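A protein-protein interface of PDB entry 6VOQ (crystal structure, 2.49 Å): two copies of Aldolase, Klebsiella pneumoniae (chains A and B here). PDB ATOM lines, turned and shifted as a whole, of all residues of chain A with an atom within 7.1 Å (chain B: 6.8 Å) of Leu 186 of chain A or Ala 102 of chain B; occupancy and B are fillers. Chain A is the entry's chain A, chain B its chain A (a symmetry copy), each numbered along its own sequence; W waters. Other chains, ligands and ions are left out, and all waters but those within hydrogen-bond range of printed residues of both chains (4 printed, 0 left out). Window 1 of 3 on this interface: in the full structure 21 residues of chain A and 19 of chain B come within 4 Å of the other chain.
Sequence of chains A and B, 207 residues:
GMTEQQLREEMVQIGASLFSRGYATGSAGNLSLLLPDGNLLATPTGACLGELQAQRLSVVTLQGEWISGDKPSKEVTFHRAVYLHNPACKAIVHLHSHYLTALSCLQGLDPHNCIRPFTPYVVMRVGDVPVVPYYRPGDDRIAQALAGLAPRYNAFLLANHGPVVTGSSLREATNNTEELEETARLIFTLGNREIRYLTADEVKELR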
ATOM      1  N   TYR A  99      12.977 -18.156  39.174  1.00  0.00           N
ATOM      2  CA  TYR A  99      13.749 -17.830  37.985  1.00  0.00           C
ATOM      3  C   TYR A  99      13.431 -16.440  37.451  1.00  0.00           C
ATOM      4  O   TYR A  99      14.325 -15.776  36.918  1.00  0.00           O
ATOM      5  CB  TYR A  99      13.548 -18.922  36.927  1.00  0.00           C
ATOM      6  CG  TYR A  99      14.118 -20.234  37.426  1.00  0.00           C
ATOM      7  CD1 TYR A  99      15.483 -20.479  37.384  1.00  0.00           C
ATOM      8  CD2 TYR A  99      13.299 -21.197  38.009  1.00  0.00           C
ATOM      9  CE1 TYR A  99      16.012 -21.665  37.880  1.00  0.00           C
ATOM     10  CE2 TYR A  99      13.819 -22.382  38.493  1.00  0.00           C
ATOM     11  CZ  TYR A  99      15.174 -22.602  38.431  1.00  0.00           C
ATOM     12  OH  TYR A  99      15.695 -23.776  38.917  1.00  0.00           O
ATOM     13  N   PHE A 118      12.510 -17.679  22.696  1.00  0.00           N
ATOM     14  CA  PHE A 118      12.813 -18.950  22.048  1.00  0.00           C
ATOM     15  C   PHE A 118      11.638 -19.915  22.106  1.00  0.00           C
ATOM     16  O   PHE A 118      11.788 -21.068  21.704  1.00  0.00           O
ATOM     17  CB  PHE A 118      14.035 -19.621  22.696  1.00  0.00           C
ATOM     18  CG  PHE A 118      13.996 -19.620  24.195  1.00  0.00           C
ATOM     19  CD1 PHE A 118      13.258 -20.575  24.887  1.00  0.00           C
ATOM     20  CD2 PHE A 118      14.677 -18.650  24.917  1.00  0.00           C
ATOM     21  CE1 PHE A 118      13.208 -20.569  26.277  1.00  0.00           C
ATOM     22  CE2 PHE A 118      14.637 -18.641  26.305  1.00  0.00           C
ATOM     23  CZ  PHE A 118      13.896 -19.598  26.988  1.00  0.00           C
ATOM     24  N   THR A 119      10.500 -19.492  22.646  1.00  0.00           N
ATOM     25  CA  THR A 119       9.240 -20.218  22.628  1.00  0.00           C
ATOM     26  C   THR A 119       8.155 -19.209  22.331  1.00  0.00           C
ATOM     27  O   THR A 119       8.288 -18.027  22.676  1.00  0.00           O
ATOM     28  CB  THR A 119       8.946 -20.909  23.962  1.00  0.00           C
ATOM     29  OG1 THR A 119       9.177 -19.984  25.033  1.00  0.00           O
ATOM     30  CG2 THR A 119       9.832 -22.121  24.134  1.00  0.00           C
ATOM     31  N   GLU A 179       3.544 -19.164  32.795  1.00  0.00           N
ATOM     32  CA  GLU A 179       4.235 -19.207  31.514  1.00  0.00           C
ATOM     33  C   GLU A 179       5.516 -18.381  31.555  1.00  0.00           C
ATOM     34  O   GLU A 179       6.557 -18.817  31.055  1.00  0.00           O
ATOM     35  CB  GLU A 179       3.304 -18.723  30.405  1.00  0.00           C
ATOM     36  CG  GLU A 179       3.850 -18.944  29.007  1.00  0.00           C
ATOM     37  CD  GLU A 179       4.003 -20.417  28.671  1.00  0.00           C
ATOM     38  OE1 GLU A 179       3.086 -21.205  29.003  1.00  0.00           O
ATOM     39  OE2 GLU A 179       5.049 -20.788  28.088  1.00  0.00           O
ATOM     40  N   LEU A 180       5.465 -17.197  32.168  1.00  0.00           N
ATOM     41  CA  LEU A 180       6.657 -16.367  32.271  1.00  0.00           C
ATOM     42  C   LEU A 180       7.727 -17.046  33.111  1.00  0.00           C
ATOM     43  O   LEU A 180       8.905 -17.053  32.738  1.00  0.00           O
ATOM     44  CB  LEU A 180       6.306 -15.014  32.874  1.00  0.00           C
ATOM     45  CG  LEU A 180       5.855 -13.950  31.903  1.00  0.00           C
ATOM     46  CD1 LEU A 180       5.207 -12.829  32.700  1.00  0.00           C
ATOM     47  CD2 LEU A 180       7.048 -13.462  31.076  1.00  0.00           C
ATOM     48  N   GLU A 181       7.338 -17.602  34.263  1.00  0.00           N
ATOM     49  CA  GLU A 181       8.321 -18.228  35.138  1.00  0.00           C
ATOM     50  C   GLU A 181       8.979 -19.411  34.448  1.00  0.00           C
ATOM     51  O   GLU A 181      10.202 -19.583  34.518  1.00  0.00           O
ATOM     52  CB  GLU A 181       7.656 -18.650  36.447  1.00  0.00           C
ATOM     53  CG  GLU A 181       8.499 -19.560  37.324  1.00  0.00           C
ATOM     54  CD  GLU A 181       9.693 -18.863  37.979  1.00  0.00           C
ATOM     55  OE1 GLU A 181       9.818 -17.619  37.905  1.00  0.00           O
ATOM     56  OE2 GLU A 181      10.511 -19.576  38.585  1.00  0.00           O
ATOM     57  N   GLU A 182       8.182 -20.214  33.743  1.00  0.00           N
ATOM     58  CA  GLU A 182       8.707 -21.334  32.976  1.00  0.00           C
ATOM     59  C   GLU A 182       9.676 -20.867  31.897  1.00  0.00           C
ATOM     60  O   GLU A 182      10.685 -21.528  31.625  1.00  0.00           O
ATOM     61  CB  GLU A 182       7.543 -22.107  32.364  1.00  0.00           C
ATOM     62  CG  GLU A 182       7.952 -23.249  31.496  1.00  0.00           C
ATOM     63  CD  GLU A 182       8.680 -24.327  32.269  1.00  0.00           C
ATOM     64  OE1 GLU A 182       9.478 -25.045  31.636  1.00  0.00           O
ATOM     65  OE2 GLU A 182       8.459 -24.450  33.496  1.00  0.00           O
ATOM     66  N   THR A 183       9.391 -19.726  31.272  1.00  0.00           N
ATOM     67  CA  THR A 183      10.303 -19.193  30.268  1.00  0.00           C
ATOM     68  C   THR A 183      11.590 -18.675  30.905  1.00  0.00           C
ATOM     69  O   THR A 183      12.684 -18.917  30.388  1.00  0.00           O
ATOM     70  CB  THR A 183       9.607 -18.100  29.459  1.00  0.00           C
ATOM     71  OG1 THR A 183       8.558 -18.693  28.684  1.00  0.00           O
ATOM     72  CG2 THR A 183      10.589 -17.430  28.513  1.00  0.00           C
ATOM     73  N   ALA A 184      11.481 -17.978  32.035  1.00  0.00           N
ATOM     74  CA  ALA A 184      12.672 -17.569  32.766  1.00  0.00           C
ATOM     75  C   ALA A 184      13.474 -18.781  33.215  1.00  0.00           C
ATOM     76  O   ALA A 184      14.703 -18.798  33.108  1.00  0.00           O
ATOM     77  CB  ALA A 184      12.279 -16.704  33.966  1.00  0.00           C
ATOM     78  N   ARG A 185      12.790 -19.821  33.681  1.00  0.00           N
ATOM     79  CA  ARG A 185      13.489 -21.029  34.088  1.00  0.00           C
ATOM     80  C   ARG A 185      14.237 -21.652  32.910  1.00  0.00           C
ATOM     81  O   ARG A 185      15.356 -22.159  33.065  1.00  0.00           O
ATOM     82  CB  ARG A 185      12.489 -22.011  34.697  1.00  0.00           C
ATOM     83  CG  ARG A 185      13.127 -23.275  35.243  1.00  0.00           C
ATOM     84  CD  ARG A 185      12.080 -24.245  35.692  1.00  0.00           C
ATOM     85  NE  ARG A 185      12.657 -25.482  36.184  1.00  0.00           N
ATOM     86  CZ  ARG A 185      11.971 -26.617  36.278  1.00  0.00           C
ATOM     87  NH1 ARG A 185      10.704 -26.649  35.904  1.00  0.00           N
ATOM     88  NH2 ARG A 185      12.549 -27.714  36.735  1.00  0.00           N
ATOM     89  N   LEU A 186      13.637 -21.616  31.723  1.00  0.00           N
ATOM     90  CA  LEU A 186      14.301 -22.174  30.558  1.00  0.00           C
ATOM     91  C   LEU A 186      15.581 -21.422  30.241  1.00  0.00           C
ATOM     92  O   LEU A 186      16.561 -22.033  29.802  1.00  0.00           O
ATOM     93  CB  LEU A 186      13.364 -22.144  29.357  1.00  0.00           C
ATOM     94  CG  LEU A 186      12.312 -23.234  29.381  1.00  0.00           C
ATOM     95  CD1 LEU A 186      11.190 -22.873  28.426  1.00  0.00           C
ATOM     96  CD2 LEU A 186      12.967 -24.545  29.005  1.00  0.00           C
ATOM     97  N   ILE A 187      15.588 -20.104  30.457  1.00  0.00           N
ATOM     98  CA  ILE A 187      16.803 -19.324  30.252  1.00  0.00           C
ATOM     99  C   ILE A 187      17.943 -19.907  31.078  1.00  0.00           C
ATOM    100  O   ILE A 187      19.016 -20.224  30.554  1.00  0.00           O
ATOM    101  CB  ILE A 187      16.544 -17.844  30.584  1.00  0.00           C
ATOM    102  CG1 ILE A 187      15.594 -17.239  29.553  1.00  0.00           C
ATOM    103  CG2 ILE A 187      17.843 -17.050  30.608  1.00  0.00           C
ATOM    104  CD1 ILE A 187      15.115 -15.846  29.884  1.00  0.00           C
ATOM    105  N   PHE A 188      17.713 -20.114  32.374  1.00  0.00           N
ATOM    106  CA  PHE A 188      18.797 -20.601  33.219  1.00  0.00           C
ATOM    107  C   PHE A 188      19.117 -22.056  32.946  1.00  0.00           C
ATOM    108  O   PHE A 188      20.273 -22.464  33.080  1.00  0.00           O
ATOM    109  CB  PHE A 188      18.459 -20.371  34.685  1.00  0.00           C
ATOM    110  CG  PHE A 188      18.543 -18.932  35.070  1.00  0.00           C
ATOM    111  CD1 PHE A 188      19.759 -18.367  35.410  1.00  0.00           C
ATOM    112  CD2 PHE A 188      17.414 -18.127  35.026  1.00  0.00           C
ATOM    113  CE1 PHE A 188      19.840 -17.029  35.745  1.00  0.00           C
ATOM    114  CE2 PHE A 188      17.484 -16.804  35.358  1.00  0.00           C
ATOM    115  CZ  PHE A 188      18.701 -16.245  35.724  1.00  0.00           C
ATOM    116  N   THR A 189      18.125 -22.835  32.517  1.00  0.00           N
ATOM    117  CA  THR A 189      18.380 -24.217  32.127  1.00  0.00           C
ATOM    118  C   THR A 189      19.229 -24.287  30.863  1.00  0.00           C
ATOM    119  O   THR A 189      20.169 -25.084  30.770  1.00  0.00           O
ATOM    120  CB  THR A 189      17.053 -24.943  31.912  1.00  0.00           C
ATOM    121  OG1 THR A 189      16.353 -25.035  33.161  1.00  0.00           O
ATOM    122  CG2 THR A 189      17.287 -26.345  31.344  1.00  0.00           C
ATOM    123  N   LEU A 190      18.891 -23.474  29.865  1.00  0.00           N
ATOM    124  CA  LEU A 190      19.644 -23.510  28.622  1.00  0.00           C
ATOM    125  C   LEU A 190      21.056 -22.995  28.822  1.00  0.00           C
ATOM    126  O   LEU A 190      21.986 -23.501  28.188  1.00  0.00           O
ATOM    127  CB  LEU A 190      18.912 -22.714  27.547  1.00  0.00           C
ATOM    128  CG  LEU A 190      17.608 -23.386  27.104  1.00  0.00           C
ATOM    129  CD1 LEU A 190      16.726 -22.425  26.316  1.00  0.00           C
ATOM    130  CD2 LEU A 190      17.935 -24.625  26.286  1.00  0.00           C
ATOM    131  N   GLY A 191      21.236 -22.022  29.717  1.00  0.00           N
ATOM    132  CA  GLY A 191      22.578 -21.591  30.070  1.00  0.00           C
ATOM    133  C   GLY A 191      23.313 -21.022  28.874  1.00  0.00           C
ATOM    134  O   GLY A 191      22.768 -20.232  28.098  1.00  0.00           O
ATOM    135  N   ILE A 195      21.219 -21.630  21.505  1.00  0.00           N
ATOM    136  CA  ILE A 195      19.765 -21.676  21.498  1.00  0.00           C
ATOM    137  C   ILE A 195      19.262 -21.322  20.107  1.00  0.00           C
ATOM    138  O   ILE A 195      19.770 -20.390  19.467  1.00  0.00           O
ATOM    139  CB  ILE A 195      19.208 -20.713  22.561  1.00  0.00           C
ATOM    140  CG1 ILE A 195      19.696 -21.154  23.940  1.00  0.00           C
ATOM    141  CG2 ILE A 195      17.672 -20.619  22.496  1.00  0.00           C
ATOM    142  CD1 ILE A 195      19.516 -20.136  25.002  1.00  0.00           C
ATOM    143  N   HIS B  96       4.516 -29.445  27.843  1.00  0.00           N
ATOM    144  CA  HIS B  96       5.692 -28.589  27.749  1.00  0.00           C
ATOM    145  C   HIS B  96       6.615 -28.844  28.926  1.00  0.00           C
ATOM    146  O   HIS B  96       7.059 -27.899  29.588  1.00  0.00           O
ATOM    147  CB  HIS B  96       5.293 -27.119  27.673  1.00  0.00           C
ATOM    148  CG  HIS B  96       4.350 -26.806  26.556  1.00  0.00           C
ATOM    149  ND1 HIS B  96       3.839 -25.543  26.345  1.00  0.00           N
ATOM    150  CD2 HIS B  96       3.820 -27.590  25.589  1.00  0.00           C
ATOM    151  CE1 HIS B  96       3.029 -25.564  25.303  1.00  0.00           C
ATOM    152  NE2 HIS B  96       3.000 -26.795  24.826  1.00  0.00           N
ATOM    153  N   SER B  97       6.882 -30.118  29.225  1.00  0.00           N
ATOM    154  CA  SER B  97       7.681 -30.443  30.400  1.00  0.00           C
ATOM    155  C   SER B  97       9.072 -29.838  30.245  1.00  0.00           C
ATOM    156  O   SER B  97       9.604 -29.737  29.134  1.00  0.00           O
ATOM    157  CB  SER B  97       7.737 -31.962  30.624  1.00  0.00           C
ATOM    158  OG  SER B  97       8.260 -32.673  29.506  1.00  0.00           O
ATOM    159  N   HIS B  98       9.642 -29.398  31.368  1.00  0.00           N
ATOM    160  CA  HIS B  98      10.666 -28.360  31.319  1.00  0.00           C
ATOM    161  C   HIS B  98      11.884 -28.798  30.509  1.00  0.00           C
ATOM    162  O   HIS B  98      12.304 -28.112  29.568  1.00  0.00           O
ATOM    163  CB  HIS B  98      11.087 -27.956  32.727  1.00  0.00           C
ATOM    164  CG  HIS B  98      12.178 -26.941  32.729  1.00  0.00           C
ATOM    165  ND1 HIS B  98      11.960 -25.617  32.408  1.00  0.00           N
ATOM    166  CD2 HIS B  98      13.515 -27.074  32.904  1.00  0.00           C
ATOM    167  CE1 HIS B  98      13.110 -24.966  32.442  1.00  0.00           C
ATOM    168  NE2 HIS B  98      14.069 -25.827  32.736  1.00  0.00           N
ATOM    169  N   TYR B  99      12.469 -29.941  30.862  1.00  0.00           N
ATOM    170  CA  TYR B  99      13.732 -30.325  30.250  1.00  0.00           C
ATOM    171  C   TYR B  99      13.554 -30.843  28.830  1.00  0.00           C
ATOM    172  O   TYR B  99      14.433 -30.626  27.991  1.00  0.00           O
ATOM    173  CB  TYR B  99      14.455 -31.332  31.153  1.00  0.00           C
ATOM    174  CG  TYR B  99      14.830 -30.673  32.465  1.00  0.00           C
ATOM    175  CD1 TYR B  99      15.935 -29.840  32.551  1.00  0.00           C
ATOM    176  CD2 TYR B  99      14.035 -30.823  33.597  1.00  0.00           C
ATOM    177  CE1 TYR B  99      16.257 -29.200  33.743  1.00  0.00           C
ATOM    178  CE2 TYR B  99      14.356 -30.199  34.786  1.00  0.00           C
ATOM    179  CZ  TYR B  99      15.462 -29.386  34.846  1.00  0.00           C
ATOM    180  OH  TYR B  99      15.781 -28.759  36.026  1.00  0.00           O
ATOM    181  N   LEU B 100      12.429 -31.492  28.520  1.00  0.00           N
ATOM    182  CA  LEU B 100      12.198 -31.865  27.130  1.00  0.00           C
ATOM    183  C   LEU B 100      11.943 -30.636  26.272  1.00  0.00           C
ATOM    184  O   LEU B 100      12.380 -30.594  25.117  1.00  0.00           O
ATOM    185  CB  LEU B 100      11.037 -32.854  27.029  1.00  0.00           C
ATOM    186  CG  LEU B 100      11.396 -34.319  27.303  1.00  0.00           C
ATOM    187  CD1 LEU B 100      10.133 -35.155  27.504  1.00  0.00           C
ATOM    188  CD2 LEU B 100      12.262 -34.907  26.184  1.00  0.00           C
ATOM    189  N   THR B 101      11.257 -29.623  26.822  1.00  0.00           N
ATOM    190  CA  THR B 101      11.090 -28.362  26.108  1.00  0.00           C
ATOM    191  C   THR B 101      12.428 -27.652  25.937  1.00  0.00           C
ATOM    192  O   THR B 101      12.706 -27.087  24.872  1.00  0.00           O
ATOM    193  CB  THR B 101      10.110 -27.449  26.856  1.00  0.00           C
ATOM    194  OG1 THR B 101       8.818 -28.063  26.932  1.00  0.00           O
ATOM    195  CG2 THR B 101       9.985 -26.086  26.164  1.00  0.00           C
ATOM    196  N   ALA B 102      13.249 -27.641  26.993  1.00  0.00           N
ATOM    197  CA  ALA B 102      14.583 -27.059  26.902  1.00  0.00           C
ATOM    198  C   ALA B 102      15.378 -27.722  25.792  1.00  0.00           C
ATOM    199  O   ALA B 102      15.911 -27.048  24.903  1.00  0.00           O
ATOM    200  CB  ALA B 102      15.319 -27.203  28.231  1.00  0.00           C
ATOM    201  N   LEU B 103      15.451 -29.052  25.827  1.00  0.00           N
ATOM    202  CA  LEU B 103      16.099 -29.794  24.757  1.00  0.00           C
ATOM    203  C   LEU B 103      15.556 -29.399  23.391  1.00  0.00           C
ATOM    204  O   LEU B 103      16.309 -29.376  22.408  1.00  0.00           O
ATOM    205  CB  LEU B 103      15.920 -31.289  24.994  1.00  0.00           C
ATOM    206  CG  LEU B 103      16.630 -32.235  24.038  1.00  0.00           C
ATOM    207  CD1 LEU B 103      18.129 -32.160  24.236  1.00  0.00           C
ATOM    208  CD2 LEU B 103      16.142 -33.624  24.294  1.00  0.00           C
ATOM    209  N   SER B 104      14.266 -29.065  23.309  1.00  0.00           N
ATOM    210  CA  SER B 104      13.656 -28.754  22.018  1.00  0.00           C
ATOM    211  C   SER B 104      14.067 -27.387  21.491  1.00  0.00           C
ATOM    212  O   SER B 104      13.877 -27.124  20.301  1.00  0.00           O
ATOM    213  CB  SER B 104      12.126 -28.822  22.117  1.00  0.00           C
ATOM    214  OG  SER B 104      11.573 -27.543  22.400  1.00  0.00           O
ATOM    215  N   CYS B 105      14.616 -26.518  22.341  1.00  0.00           N
ATOM    216  CA  CYS B 105      15.072 -25.194  21.931  1.00  0.00           C
ATOM    217  C   CYS B 105      16.550 -25.145  21.579  1.00  0.00           C
ATOM    218  O   CYS B 105      17.055 -24.066  21.263  1.00  0.00           O
ATOM    219  CB  CYS B 105      14.783 -24.157  23.028  1.00  0.00           C
ATOM    220  SG  CYS B 105      13.078 -24.128  23.597  1.00  0.00           S
ATOM    221  N   LEU B 106      17.250 -26.270  21.618  1.00  0.00           N
ATOM    222  CA  LEU B 106      18.678 -26.269  21.356  1.00  0.00           C
ATOM    223  C   LEU B 106      18.960 -26.288  19.856  1.00  0.00           C
ATOM    224  O   LEU B 106      18.171 -26.786  19.048  1.00  0.00           O
ATOM    225  CB  LEU B 106      19.352 -27.467  22.031  1.00  0.00           C
ATOM    226  CG  LEU B 106      19.521 -27.319  23.548  1.00  0.00           C
ATOM    227  CD1 LEU B 106      20.320 -28.470  24.166  1.00  0.00           C
ATOM    228  CD2 LEU B 106      20.158 -25.992  23.860  1.00  0.00           C
ATOM    229  N   LEU B 109      20.432 -30.161  17.198  1.00  0.00           N
ATOM    230  CA  LEU B 109      19.874 -31.456  17.570  1.00  0.00           C
ATOM    231  C   LEU B 109      19.908 -32.424  16.395  1.00  0.00           C
ATOM    232  O   LEU B 109      19.663 -32.046  15.247  1.00  0.00           O
ATOM    233  CB  LEU B 109      18.431 -31.302  18.036  1.00  0.00           C
ATOM    234  CG  LEU B 109      18.120 -30.601  19.352  1.00  0.00           C
ATOM    235  CD1 LEU B 109      16.626 -30.652  19.526  1.00  0.00           C
ATOM    236  CD2 LEU B 109      18.846 -31.270  20.529  1.00  0.00           C
ATOM    237  N   LEU B 157       9.803 -34.810  19.325  1.00  0.00           N
ATOM    238  CA  LEU B 157      10.149 -33.546  19.960  1.00  0.00           C
ATOM    239  C   LEU B 157       9.853 -32.434  18.965  1.00  0.00           C
ATOM    240  O   LEU B 157      10.505 -32.346  17.915  1.00  0.00           O
ATOM    241  CB  LEU B 157      11.603 -33.533  20.413  1.00  0.00           C
ATOM    242  CG  LEU B 157      12.058 -32.385  21.315  1.00  0.00           C
ATOM    243  CD1 LEU B 157      11.216 -32.296  22.566  1.00  0.00           C
ATOM    244  CD2 LEU B 157      13.514 -32.559  21.690  1.00  0.00           C
ATOM    245  N   HIS B 161       9.184 -26.068  21.547  1.00  0.00           N
ATOM    246  CA  HIS B 161       7.809 -26.370  21.900  1.00  0.00           C
ATOM    247  C   HIS B 161       7.734 -27.387  23.026  1.00  0.00           C
ATOM    248  O   HIS B 161       7.488 -27.016  24.179  1.00  0.00           O
ATOM    249  CB  HIS B 161       7.065 -26.874  20.672  1.00  0.00           C
ATOM    250  CG  HIS B 161       5.587 -26.982  20.867  1.00  0.00           C
ATOM    251  ND1 HIS B 161       4.705 -27.060  19.812  1.00  0.00           N
ATOM    252  CD2 HIS B 161       4.836 -27.019  21.990  1.00  0.00           C
ATOM    253  CE1 HIS B 161       3.474 -27.145  20.279  1.00  0.00           C
ATOM    254  NE2 HIS B 161       3.527 -27.122  21.598  1.00  0.00           N
ATOM    255  N   GLY B 162       7.924 -28.671  22.702  1.00  0.00           N
ATOM    256  CA  GLY B 162       7.851 -29.724  23.689  1.00  0.00           C
ATOM    257  C   GLY B 162       7.569 -31.105  23.115  1.00  0.00           C
ATOM    258  O   GLY B 162       7.427 -31.284  21.897  1.00  0.00           O
ATOM    259  N   GLU B 181      11.168 -37.281  30.051  1.00  0.00           N
ATOM    260  CA  GLU B 181      11.486 -36.023  30.714  1.00  0.00           C
ATOM    261  C   GLU B 181      12.646 -36.202  31.680  1.00  0.00           C
ATOM    262  O   GLU B 181      13.560 -35.370  31.730  1.00  0.00           O
ATOM    263  CB  GLU B 181      10.248 -35.486  31.429  1.00  0.00           C
ATOM    264  CG  GLU B 181      10.515 -34.335  32.385  1.00  0.00           C
ATOM    265  CD  GLU B 181      10.872 -33.019  31.692  1.00  0.00           C
ATOM    266  OE1 GLU B 181      10.769 -32.911  30.449  1.00  0.00           O
ATOM    267  OE2 GLU B 181      11.250 -32.078  32.410  1.00  0.00           O
ATOM    268  N   PHE B 188      20.681 -32.184  31.070  1.00  0.00           N
ATOM    269  CA  PHE B 188      21.067 -30.873  31.581  1.00  0.00           C
ATOM    270  C   PHE B 188      21.764 -30.972  32.922  1.00  0.00           C
ATOM    271  O   PHE B 188      22.634 -30.151  33.221  1.00  0.00           O
ATOM    272  CB  PHE B 188      19.851 -29.962  31.651  1.00  0.00           C
ATOM    273  CG  PHE B 188      19.393 -29.519  30.302  1.00  0.00           C
ATOM    274  CD1 PHE B 188      19.989 -28.436  29.680  1.00  0.00           C
ATOM    275  CD2 PHE B 188      18.410 -30.227  29.627  1.00  0.00           C
ATOM    276  CE1 PHE B 188      19.579 -28.040  28.422  1.00  0.00           C
ATOM    277  CE2 PHE B 188      17.996 -29.840  28.384  1.00  0.00           C
ATOM    278  CZ  PHE B 188      18.579 -28.738  27.772  1.00  0.00           C
HETATM  279  O   HOH W   1       4.872 -23.853  28.799  1.00  0.00           O
HETATM  280  O   HOH W   2       8.378 -25.584  29.351  1.00  0.00           O
HETATM  281  O   HOH W   3      15.607 -25.856  37.124  1.00  0.00           O
HETATM  282  O   HOH W   4       6.993 -27.480  32.634  1.00  0.00           O
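N of His 98 of chain B lies within hydrogen-bond range of OE2 of Glu 181 of chain B, 3.3 Å away.
The side-chain carboxylate of Glu 182 of chain A is in salt-bridge range of the guanidinium group of Arg 185 of chain A, at 3.96 Å.
The side-chain carboxylate (OE2) of Glu 181 of chain B lies within hydrogen-bond range of the backbone NH (N) of Tyr 99 of chain B.
O of Arg 185 of chain A sits at hydrogen-bond distance from OG1 of Thr 189 of chain A (3.0 Å).
The backbone carbonyl oxygen (O) of Thr 101 of chain B sits at hydrogen-bond distance from the side-chain sulfur (SG) of Cys 105 of chain B (3.2 Å).
SG of Cys 105 of chain B touches CD1 of Phe 118 of chain A (3.8 Å).
SG of Cys 105 of chain B touches CG2 of Thr 119 of chain A, 3.9 Å away.
Arg 185 of chain A touches His 98 of chain B.
CB of Ala 102 of chain B touches CD2 of Leu 186 of chain A, at 3.6 Å.
Tyr 99 of chain B touches Thr 189 of chain A (CE1 to CG2, 3.9 Å).
CG2 of Thr 189 of chain A touches CB of Ala 102 of chain B, 3.8 Å away.
Thr 189 of chain A touches Phe 188 of chain B.
Leu 190 of chain A touches Ala 102 of chain B (CD2 to O, 3.4 Å).
Leu 106 of chain B touches Leu 190 of chain A.
Cys 105 of chain B touches Ile 195 of chain A (O to CA, 3.6 Å).
Positions printed for both chains: 99, 181 and 188.
Of the 14 pairs that touch across the chains among the printed residues, none has its exchanged pair printed and touching as well.
Water W2 lies within hydrogen-bond range of OE1 of Glu 182 of chain A, O of His 96 of chain B and OG1 of Thr 101 of chain B.
Water W3 lies within hydrogen-bond range of OH of Tyr 99 of chain A (2.7 Å), OH of Tyr 99 of chain B (3.1 Å) and NE of Arg 185 of chain A (3.1 Å).
Water W4 lies within hydrogen-bond range of O of His 96 of chain B (3.1 Å) and OE2 of Glu 182 of chain A (3.5 Å).
Water W1 bridges the side-chain carboxylate (OE2) of Glu 179 of chain A (3.2 Å) and a ring nitrogen (ND1) of His 96 of chain B (3.2 Å).
Printed residues of chain B within 4 Å of Thr 119 of chain A: Cys 105.
Glu 179 of chain A touches none of the printed residues of chain B.
Of the printed residues of chain B, Glu 182 of chain A touches His 98.
Of chain B, only His 98 (3.5 Å) and Ala 102 (3.6 Å) come within 4 Å of Leu 186 of chain A.
Of the printed residues of chain A, His 98 of chain B touches Glu 182 (2.7 Å), Arg 185 (3.3 Å), Leu 186 (3.5 Å) and Thr 189 (2.5 Å).
Ala 102 of chain B touches just these residues of chain A: Leu 186 (3.6 Å), Thr 189 (3.8 Å) and Leu 190 (3.4 Å).
The nearest residue of chain A that does not touch Ala 102 of chain B is Glu 182 of chain A (6.5 Å).
The nearest printed residue of chain A that does not touch Phe 188 of chain B is Leu 190 of chain A (4.4 Å).
ND1 of His 98 of chain B is in hydrogen-bond range of OE1 of Glu 182 of chain A (2.7 Å).
OG1 of Thr 189 of chain A is in hydrogen-bond range of NE2 of His 98 of chain B, at 2.5 Å.
The guanidinium group (NH2) of Arg 185 of chain A lies within hydrogen-bond range of the side-chain hydroxyl (OH) of Tyr 99 of chain B (3.5 Å).
Of the 17 printed residues of chain B, 6 touch a printed residue of chain A.
Of the 17 printed residues of chain A, 8 touch a printed residue of chain B.
Among the printed residues, no Asp or Glu carboxylate lies within 4 Å of a Lys or Arg side-chain nitrogen of the other chain.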
